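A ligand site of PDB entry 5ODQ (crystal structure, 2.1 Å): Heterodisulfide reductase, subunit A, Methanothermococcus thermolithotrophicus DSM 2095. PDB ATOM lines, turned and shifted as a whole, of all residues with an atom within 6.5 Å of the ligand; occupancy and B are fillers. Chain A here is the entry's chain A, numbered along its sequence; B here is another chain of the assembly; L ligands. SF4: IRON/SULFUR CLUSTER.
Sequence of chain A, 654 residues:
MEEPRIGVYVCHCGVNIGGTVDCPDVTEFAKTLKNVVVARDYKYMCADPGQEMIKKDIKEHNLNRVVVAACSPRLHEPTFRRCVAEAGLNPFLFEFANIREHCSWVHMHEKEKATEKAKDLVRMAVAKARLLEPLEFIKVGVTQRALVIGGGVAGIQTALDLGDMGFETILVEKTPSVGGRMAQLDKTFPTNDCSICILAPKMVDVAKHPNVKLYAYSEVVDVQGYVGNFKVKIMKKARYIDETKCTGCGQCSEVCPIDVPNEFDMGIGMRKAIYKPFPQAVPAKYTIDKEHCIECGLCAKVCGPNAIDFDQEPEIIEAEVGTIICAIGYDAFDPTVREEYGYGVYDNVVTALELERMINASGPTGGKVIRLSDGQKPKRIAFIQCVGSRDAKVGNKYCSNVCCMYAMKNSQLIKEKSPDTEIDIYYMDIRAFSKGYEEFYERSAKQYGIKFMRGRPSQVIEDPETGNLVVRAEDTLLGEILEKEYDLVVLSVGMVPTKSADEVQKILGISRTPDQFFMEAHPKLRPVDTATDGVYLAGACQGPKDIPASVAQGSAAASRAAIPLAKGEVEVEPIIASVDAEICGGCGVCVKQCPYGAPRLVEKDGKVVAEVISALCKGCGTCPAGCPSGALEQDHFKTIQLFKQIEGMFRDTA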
ATOM      1  N   ILE A 384      -0.805  -3.558  24.635  1.00  0.00           N
ATOM      2  CA  ILE A 384      -1.708  -2.835  23.756  1.00  0.00           C
ATOM      3  C   ILE A 384      -3.037  -3.482  23.943  1.00  0.00           C
ATOM      4  O   ILE A 384      -3.192  -4.658  23.669  1.00  0.00           O
ATOM      5  CB  ILE A 384      -1.229  -2.881  22.286  1.00  0.00           C
ATOM      6  CG1 ILE A 384       0.115  -2.134  22.172  1.00  0.00           C
ATOM      7  CG2 ILE A 384      -2.298  -2.247  21.377  1.00  0.00           C
ATOM      8  CD1 ILE A 384       0.751  -2.107  20.825  1.00  0.00           C
ATOM      9  N   GLN A 385      -4.005  -2.724  24.453  1.00  0.00           N
ATOM     10  CA  GLN A 385      -5.324  -3.251  24.707  1.00  0.00           C
ATOM     11  C   GLN A 385      -6.198  -3.267  23.480  1.00  0.00           C
ATOM     12  O   GLN A 385      -5.897  -2.619  22.485  1.00  0.00           O
ATOM     13  CB  GLN A 385      -6.012  -2.469  25.838  1.00  0.00           C
ATOM     14  CG  GLN A 385      -5.239  -2.491  27.145  1.00  0.00           C
ATOM     15  CD  GLN A 385      -4.867  -3.894  27.522  1.00  0.00           C
ATOM     16  OE1 GLN A 385      -3.711  -4.313  27.361  1.00  0.00           O
ATOM     17  NE2 GLN A 385      -5.868  -4.674  27.902  1.00  0.00           N
ATOM     18  N   CYS A 386      -7.293  -4.043  23.563  1.00  0.00           N
ATOM     19  CA  CYS A 386      -8.295  -4.189  22.512  1.00  0.00           C
ATOM     20  C   CYS A 386      -7.744  -4.698  21.178  1.00  0.00           C
ATOM     21  O   CYS A 386      -8.244  -4.284  20.136  1.00  0.00           O
ATOM     22  CB  CYS A 386      -9.060  -2.884  22.348  1.00  0.00           C
ATOM     23  SG  CYS A 386      -9.709  -2.213  23.889  1.00  0.00           S
ATOM     24  N   VAL A 387      -6.747  -5.588  21.180  1.00  0.00           N
ATOM     25  CA  VAL A 387      -6.222  -6.096  19.914  1.00  0.00           C
ATOM     26  C   VAL A 387      -7.146  -7.204  19.391  1.00  0.00           C
ATOM     27  O   VAL A 387      -7.229  -8.285  19.970  1.00  0.00           O
ATOM     28  CB  VAL A 387      -4.763  -6.571  20.041  1.00  0.00           C
ATOM     29  CG1 VAL A 387      -4.277  -7.183  18.725  1.00  0.00           C
ATOM     30  CG2 VAL A 387      -3.871  -5.396  20.438  1.00  0.00           C
ATOM     31  N   SER A 389     -10.449  -6.632  19.022  1.00  0.00           N
ATOM     32  CA  SER A 389     -11.740  -6.376  19.662  1.00  0.00           C
ATOM     33  C   SER A 389     -12.089  -4.924  19.514  1.00  0.00           C
ATOM     34  O   SER A 389     -11.192  -4.089  19.347  1.00  0.00           O
ATOM     35  CB  SER A 389     -11.663  -6.709  21.144  1.00  0.00           C
ATOM     36  OG  SER A 389     -11.206  -8.028  21.369  1.00  0.00           O
ATOM     37  N   ARG A 390     -13.396  -4.589  19.573  1.00  0.00           N
ATOM     38  CA  ARG A 390     -13.837  -3.195  19.437  1.00  0.00           C
ATOM     39  C   ARG A 390     -13.178  -2.629  18.188  1.00  0.00           C
ATOM     40  O   ARG A 390     -12.725  -1.485  18.190  1.00  0.00           O
ATOM     41  CB  ARG A 390     -13.424  -2.365  20.676  1.00  0.00           C
ATOM     42  CG  ARG A 390     -13.840  -2.990  22.016  1.00  0.00           C
ATOM     43  CD  ARG A 390     -13.467  -2.106  23.200  1.00  0.00           C
ATOM     44  NE  ARG A 390     -14.079  -0.781  23.118  1.00  0.00           N
ATOM     45  CZ  ARG A 390     -13.889   0.188  23.994  1.00  0.00           C
ATOM     46  NH1 ARG A 390     -13.094  -0.003  25.039  1.00  0.00           N
ATOM     47  NH2 ARG A 390     -14.485   1.362  23.845  1.00  0.00           N
ATOM     48  N   TYR A 398     -17.027  -6.246  19.120  1.00  0.00           N
ATOM     49  CA  TYR A 398     -17.409  -6.567  20.496  1.00  0.00           C
ATOM     50  C   TYR A 398     -16.227  -6.429  21.426  1.00  0.00           C
ATOM     51  O   TYR A 398     -15.080  -6.378  20.988  1.00  0.00           O
ATOM     52  CB  TYR A 398     -17.933  -8.005  20.582  1.00  0.00           C
ATOM     53  CG  TYR A 398     -16.959  -9.039  20.052  1.00  0.00           C
ATOM     54  CD1 TYR A 398     -16.927  -9.364  18.700  1.00  0.00           C
ATOM     55  CD2 TYR A 398     -16.084  -9.703  20.893  1.00  0.00           C
ATOM     56  CE1 TYR A 398     -16.024 -10.303  18.205  1.00  0.00           C
ATOM     57  CE2 TYR A 398     -15.189 -10.648  20.416  1.00  0.00           C
ATOM     58  CZ  TYR A 398     -15.165 -10.956  19.067  1.00  0.00           C
ATOM     59  OH  TYR A 398     -14.297 -11.887  18.560  1.00  0.00           O
ATOM     60  N   CYS A 399     -16.499  -6.385  22.743  1.00  0.00           N
ATOM     61  CA  CYS A 399     -15.471  -6.290  23.765  1.00  0.00           C
ATOM     62  C   CYS A 399     -15.178  -7.735  24.163  1.00  0.00           C
ATOM     63  O   CYS A 399     -16.109  -8.504  24.383  1.00  0.00           O
ATOM     64  CB  CYS A 399     -15.944  -5.441  24.939  1.00  0.00           C
ATOM     65  SG  CYS A 399     -14.999  -5.677  26.473  1.00  0.00           S
ATOM     66  N   SER A 400     -13.880  -8.115  24.243  1.00  0.00           N
ATOM     67  CA  SER A 400     -13.519  -9.486  24.593  1.00  0.00           C
ATOM     68  C   SER A 400     -13.555  -9.742  26.088  1.00  0.00           C
ATOM     69  O   SER A 400     -13.165 -10.810  26.550  1.00  0.00           O
ATOM     70  CB  SER A 400     -12.182  -9.867  23.965  1.00  0.00           C
ATOM     71  OG  SER A 400     -12.379 -10.182  22.601  1.00  0.00           O
ATOM     72  N   ASN A 401     -14.052  -8.762  26.854  1.00  0.00           N
ATOM     73  CA  ASN A 401     -14.273  -8.855  28.294  1.00  0.00           C
ATOM     74  C   ASN A 401     -13.088  -9.090  29.260  1.00  0.00           C
ATOM     75  O   ASN A 401     -13.039  -8.425  30.293  1.00  0.00           O
ATOM     76  CB  ASN A 401     -15.285  -9.965  28.503  1.00  0.00           C
ATOM     77  CG  ASN A 401     -15.660 -10.210  29.920  1.00  0.00           C
ATOM     78  OD1 ASN A 401     -14.893 -10.784  30.690  1.00  0.00           O
ATOM     79  ND2 ASN A 401     -16.868  -9.831  30.272  1.00  0.00           N
ATOM     80  N   VAL A 402     -12.177 -10.041  28.979  1.00  0.00           N
ATOM     81  CA  VAL A 402     -11.064 -10.350  29.890  1.00  0.00           C
ATOM     82  C   VAL A 402      -9.714  -9.655  29.671  1.00  0.00           C
ATOM     83  O   VAL A 402      -8.860  -9.739  30.550  1.00  0.00           O
ATOM     84  CB  VAL A 402     -10.805 -11.877  29.839  1.00  0.00           C
ATOM     85  CG1 VAL A 402     -12.107 -12.670  30.045  1.00  0.00           C
ATOM     86  CG2 VAL A 402     -10.135 -12.264  28.527  1.00  0.00           C
ATOM     87  N   CYS A 403      -9.499  -9.020  28.534  1.00  0.00           N
ATOM     88  CA  CYS A 403      -8.206  -8.408  28.218  1.00  0.00           C
ATOM     89  C   CYS A 403      -7.742  -7.288  29.145  1.00  0.00           C
ATOM     90  O   CYS A 403      -6.538  -7.208  29.396  1.00  0.00           O
ATOM     91  CB  CYS A 403      -8.192  -7.955  26.767  1.00  0.00           C
ATOM     92  SG  CYS A 403      -9.647  -8.440  25.825  1.00  0.00           S
ATOM     93  N   CYS A 404      -8.630  -6.418  29.623  1.00  0.00           N
ATOM     94  CA  CYS A 404      -8.161  -5.359  30.520  1.00  0.00           C
ATOM     95  C   CYS A 404      -7.599  -5.983  31.766  1.00  0.00           C
ATOM     96  O   CYS A 404      -6.509  -5.626  32.210  1.00  0.00           O
ATOM     97  CB  CYS A 404      -9.287  -4.385  30.843  1.00  0.00           C
ATOM     98  SG  CYS A 404      -9.564  -3.113  29.579  1.00  0.00           S
ATOM     99  N   MET A 405      -8.333  -6.947  32.331  1.00  0.00           N
ATOM    100  CA  MET A 405      -7.921  -7.641  33.548  1.00  0.00           C
ATOM    101  C   MET A 405      -6.650  -8.496  33.380  1.00  0.00           C
ATOM    102  O   MET A 405      -5.751  -8.348  34.197  1.00  0.00           O
ATOM    103  CB  MET A 405      -9.069  -8.502  34.078  1.00  0.00           C
ATOM    104  CG  MET A 405     -10.238  -7.690  34.625  1.00  0.00           C
ATOM    105  SD  MET A 405      -9.823  -6.635  36.042  1.00  0.00           S
ATOM    106  CE  MET A 405      -9.498  -7.882  37.288  1.00  0.00           C
ATOM    107  N   MET A 428      -8.183   2.288  26.084  1.00  0.00           N
ATOM    108  CA  MET A 428      -9.283   3.194  25.729  1.00  0.00           C
ATOM    109  C   MET A 428     -10.165   3.283  26.968  1.00  0.00           C
ATOM    110  O   MET A 428     -10.452   4.371  27.449  1.00  0.00           O
ATOM    111  CB  MET A 428     -10.078   2.640  24.549  1.00  0.00           C
ATOM    112  CG  MET A 428      -9.426   2.898  23.217  1.00  0.00           C
ATOM    113  SD  MET A 428     -10.449   2.356  21.845  1.00  0.00           S
ATOM    114  CE  MET A 428     -10.245   0.635  21.956  1.00  0.00           C
ATOM    115  N   ASP A 429     -10.594   2.108  27.475  1.00  0.00           N
ATOM    116  CA  ASP A 429     -11.399   1.991  28.688  1.00  0.00           C
ATOM    117  C   ASP A 429     -10.866   0.847  29.501  1.00  0.00           C
ATOM    118  O   ASP A 429     -10.538  -0.198  28.937  1.00  0.00           O
ATOM    119  CB  ASP A 429     -12.873   1.670  28.404  1.00  0.00           C
ATOM    120  CG  ASP A 429     -13.606   2.694  27.582  1.00  0.00           C
ATOM    121  OD1 ASP A 429     -14.070   3.692  28.164  1.00  0.00           O
ATOM    122  OD2 ASP A 429     -13.832   2.434  26.383  1.00  0.00           O
ATOM    123  N   ILE A 430     -10.750   1.015  30.816  1.00  0.00           N
ATOM    124  CA  ILE A 430     -10.283  -0.055  31.670  1.00  0.00           C
ATOM    125  C   ILE A 430     -11.557  -0.670  32.174  1.00  0.00           C
ATOM    126  O   ILE A 430     -12.309  -0.010  32.876  1.00  0.00           O
ATOM    127  CB  ILE A 430      -9.406   0.442  32.832  1.00  0.00           C
ATOM    128  CG1 ILE A 430      -8.065   1.003  32.315  1.00  0.00           C
ATOM    129  CG2 ILE A 430      -9.168  -0.672  33.849  1.00  0.00           C
ATOM    130  CD1 ILE A 430      -7.139  -0.019  31.598  1.00  0.00           C
ATOM    131  N   ARG A 431     -11.816  -1.916  31.788  1.00  0.00           N
ATOM    132  CA  ARG A 431     -13.041  -2.596  32.188  1.00  0.00           C
ATOM    133  C   ARG A 431     -12.768  -3.613  33.286  1.00  0.00           C
ATOM    134  O   ARG A 431     -12.493  -4.783  33.044  1.00  0.00           O
ATOM    135  CB  ARG A 431     -13.710  -3.192  30.944  1.00  0.00           C
ATOM    136  CG  ARG A 431     -14.109  -2.065  29.989  1.00  0.00           C
ATOM    137  CD  ARG A 431     -14.873  -2.486  28.764  1.00  0.00           C
ATOM    138  NE  ARG A 431     -15.336  -1.295  28.030  1.00  0.00           N
ATOM    139  CZ  ARG A 431     -15.739  -1.286  26.769  1.00  0.00           C
ATOM    140  NH1 ARG A 431     -16.132  -0.161  26.201  1.00  0.00           N
ATOM    141  NH2 ARG A 431     -15.749  -2.413  26.062  1.00  0.00           N
ATOM    142  N   PHE A 433     -14.959  -4.400  35.867  1.00  0.00           N
ATOM    143  CA  PHE A 433     -16.388  -4.372  36.181  1.00  0.00           C
ATOM    144  C   PHE A 433     -16.936  -5.340  37.228  1.00  0.00           C
ATOM    145  O   PHE A 433     -18.110  -5.182  37.600  1.00  0.00           O
ATOM    146  CB  PHE A 433     -17.142  -4.620  34.870  1.00  0.00           C
ATOM    147  CG  PHE A 433     -16.706  -5.914  34.212  1.00  0.00           C
ATOM    148  CD1 PHE A 433     -17.223  -7.132  34.623  1.00  0.00           C
ATOM    149  CD2 PHE A 433     -15.724  -5.920  33.234  1.00  0.00           C
ATOM    150  CE1 PHE A 433     -16.796  -8.319  34.053  1.00  0.00           C
ATOM    151  CE2 PHE A 433     -15.285  -7.112  32.668  1.00  0.00           C
ATOM    152  CZ  PHE A 433     -15.836  -8.302  33.074  1.00  0.00           C
ATOM    153  N   SER A 492      -2.769  -7.531  23.622  1.00  0.00           N
ATOM    154  CA  SER A 492      -3.862  -8.123  24.377  1.00  0.00           C
ATOM    155  C   SER A 492      -4.927  -8.569  23.405  1.00  0.00           C
ATOM    156  O   SER A 492      -5.912  -7.869  23.175  1.00  0.00           O
ATOM    157  CB  SER A 492      -4.387  -7.134  25.407  1.00  0.00           C
ATOM    158  OG  SER A 492      -3.365  -6.864  26.349  1.00  0.00           O
ATOM    159  N   GLY A 494      -7.981 -10.463  21.606  1.00  0.00           N
ATOM    160  CA  GLY A 494      -9.336 -10.779  22.005  1.00  0.00           C
ATOM    161  C   GLY A 494      -9.654 -12.245  21.873  1.00  0.00           C
ATOM    162  O   GLY A 494      -8.771 -13.059  21.558  1.00  0.00           O
ATOM    163  N   ILE B 430     -16.222   3.616  29.911  1.00  0.00           N
ATOM    164  CA  ILE B 430     -17.497   3.076  29.477  1.00  0.00           C
ATOM    165  C   ILE B 430     -17.292   1.595  29.555  1.00  0.00           C
ATOM    166  O   ILE B 430     -16.468   1.064  28.824  1.00  0.00           O
ATOM    167  CB  ILE B 430     -17.886   3.528  28.052  1.00  0.00           C
ATOM    168  CG1 ILE B 430     -18.173   5.033  27.994  1.00  0.00           C
ATOM    169  CG2 ILE B 430     -19.083   2.721  27.550  1.00  0.00           C
ATOM    170  CD1 ILE B 430     -19.387   5.513  28.852  1.00  0.00           C
ATOM    171  N   ALA B 432     -18.820  -1.558  28.735  1.00  0.00           N
ATOM    172  CA  ALA B 432     -19.718  -2.293  27.860  1.00  0.00           C
ATOM    173  C   ALA B 432     -18.884  -3.523  27.534  1.00  0.00           C
ATOM    174  O   ALA B 432     -18.350  -3.680  26.446  1.00  0.00           O
ATOM    175  CB  ALA B 432     -19.966  -1.456  26.610  1.00  0.00           C
ATOM    176  N   PHE B 433     -18.768  -4.380  28.530  1.00  0.00           N
ATOM    177  CA  PHE B 433     -17.939  -5.580  28.563  1.00  0.00           C
ATOM    178  C   PHE B 433     -18.534  -6.922  28.154  1.00  0.00           C
ATOM    179  O   PHE B 433     -17.757  -7.869  28.023  1.00  0.00           O
ATOM    180  CB  PHE B 433     -17.401  -5.724  29.993  1.00  0.00           C
ATOM    181  CG  PHE B 433     -18.536  -5.775  31.002  1.00  0.00           C
ATOM    182  CD1 PHE B 433     -19.220  -6.953  31.245  1.00  0.00           C
ATOM    183  CD2 PHE B 433     -18.954  -4.628  31.653  1.00  0.00           C
ATOM    184  CE1 PHE B 433     -20.273  -6.982  32.136  1.00  0.00           C
ATOM    185  CE2 PHE B 433     -20.003  -4.666  32.543  1.00  0.00           C
ATOM    186  CZ  PHE B 433     -20.662  -5.843  32.785  1.00  0.00           C
ATOM    187  N   GLU B 438     -20.696  -3.598  23.796  1.00  0.00           N
ATOM    188  CA  GLU B 438     -19.900  -2.625  23.045  1.00  0.00           C
ATOM    189  C   GLU B 438     -20.703  -2.170  21.836  1.00  0.00           C
ATOM    190  O   GLU B 438     -20.673  -0.995  21.458  1.00  0.00           O
ATOM    191  CB  GLU B 438     -18.566  -3.267  22.600  1.00  0.00           C
ATOM    192  CG  GLU B 438     -17.677  -2.350  21.767  1.00  0.00           C
ATOM    193  CD  GLU B 438     -17.090  -1.181  22.523  1.00  0.00           C
ATOM    194  OE1 GLU B 438     -17.009  -1.245  23.769  1.00  0.00           O
ATOM    195  OE2 GLU B 438     -16.655  -0.205  21.850  1.00  0.00           O
HETATM  196 FE1  SF4 L   1     -12.767  -4.862  26.352  1.00  0.00          FE
HETATM  197 FE2  SF4 L   1     -10.607  -4.344  27.823  1.00  0.00          FE
HETATM  198 FE3  SF4 L   1     -10.625  -3.936  25.121  1.00  0.00          FE
HETATM  199 FE4  SF4 L   1     -10.502  -6.288  26.234  1.00  0.00          FE
HETATM  200  S1  SF4 L   1      -8.835  -4.716  26.358  1.00  0.00           S
HETATM  201  S2  SF4 L   1     -11.862  -5.740  24.441  1.00  0.00           S
HETATM  202  S3  SF4 L   1     -11.905  -6.219  28.078  1.00  0.00           S
HETATM  203  S4  SF4 L   1     -11.863  -2.756  26.634  1.00  0.00           S
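FE3 of the ligand is bound by SG of Cys 386 (2.3 Å). The side-chain sulfur of Cys 399 is bound to an iron atom (FE1) of the ligand, 2.4 Å away. NE2 of Gln 385 lies close to S1 of the ligand (3.3 Å). N of Cys 386 lies close to S1 of the ligand (3.3 Å). A sulfur (S3) of the ligand sits close to the backbone NH of Cys 403. The side-chain sulfur (SG) of Cys 404 binds an iron atom (FE2) of the ligand (2.4 Å). The backbone NH (N) of Ser 400 lies close to a sulfur (S2) of the ligand (3.1 Å). NH1 of Arg 390 lies close to S4 of the ligand (3.4 Å). SG of Cys 403 binds FE4 of the ligand (2.4 Å). A sulfur (S3) of the ligand sits close to the backbone NH of Cys 404 (3.6 Å). S3 of the ligand lies close to N of Asn 401 (3.5 Å).
The backbone carbonyl oxygen (O) of Asp 429 lies close to a sulfur (S4) of the ligand (3.7 Å). Residues that only touch the ligand: Ser 389 (3.4 Å), Arg 431 (3.7 Å) and Val 402 (3.9 Å). 12 residues have an atom within 4 Å of the ligand: Gln 385, Cys 386, Ser 389, Arg 390, Cys 399, Ser 400, Asn 401, Val 402, Cys 403, Cys 404, Asp 429 and Arg 431.
OG of Ser 389 is in hydrogen-bond range of OG of Ser 400 (2.7 Å). NE of Arg 431 is in hydrogen-bond range of O of Ile 430 of chain B, at 2.7 Å. NH2 of Arg 431 lies close to SG of Cys 399 (3.4 Å). O of Phe 433 of chain B sits at hydrogen-bond distance from ND2 of Asn 401, at 3.1 Å. OE1 of Gln 385 lies within hydrogen-bond range of OG of Ser 492. N of Asn 401 lies close to SG of Cys 399. The backbone carbonyl oxygen (O) of Asp 429 sits close to the side-chain sulfur (SG) of Cys 404, 3.1 Å away. The backbone carbonyl oxygen (O) of Tyr 398 lies within hydrogen-bond range of the backbone NH (N) of Arg 390 (2.8 Å).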
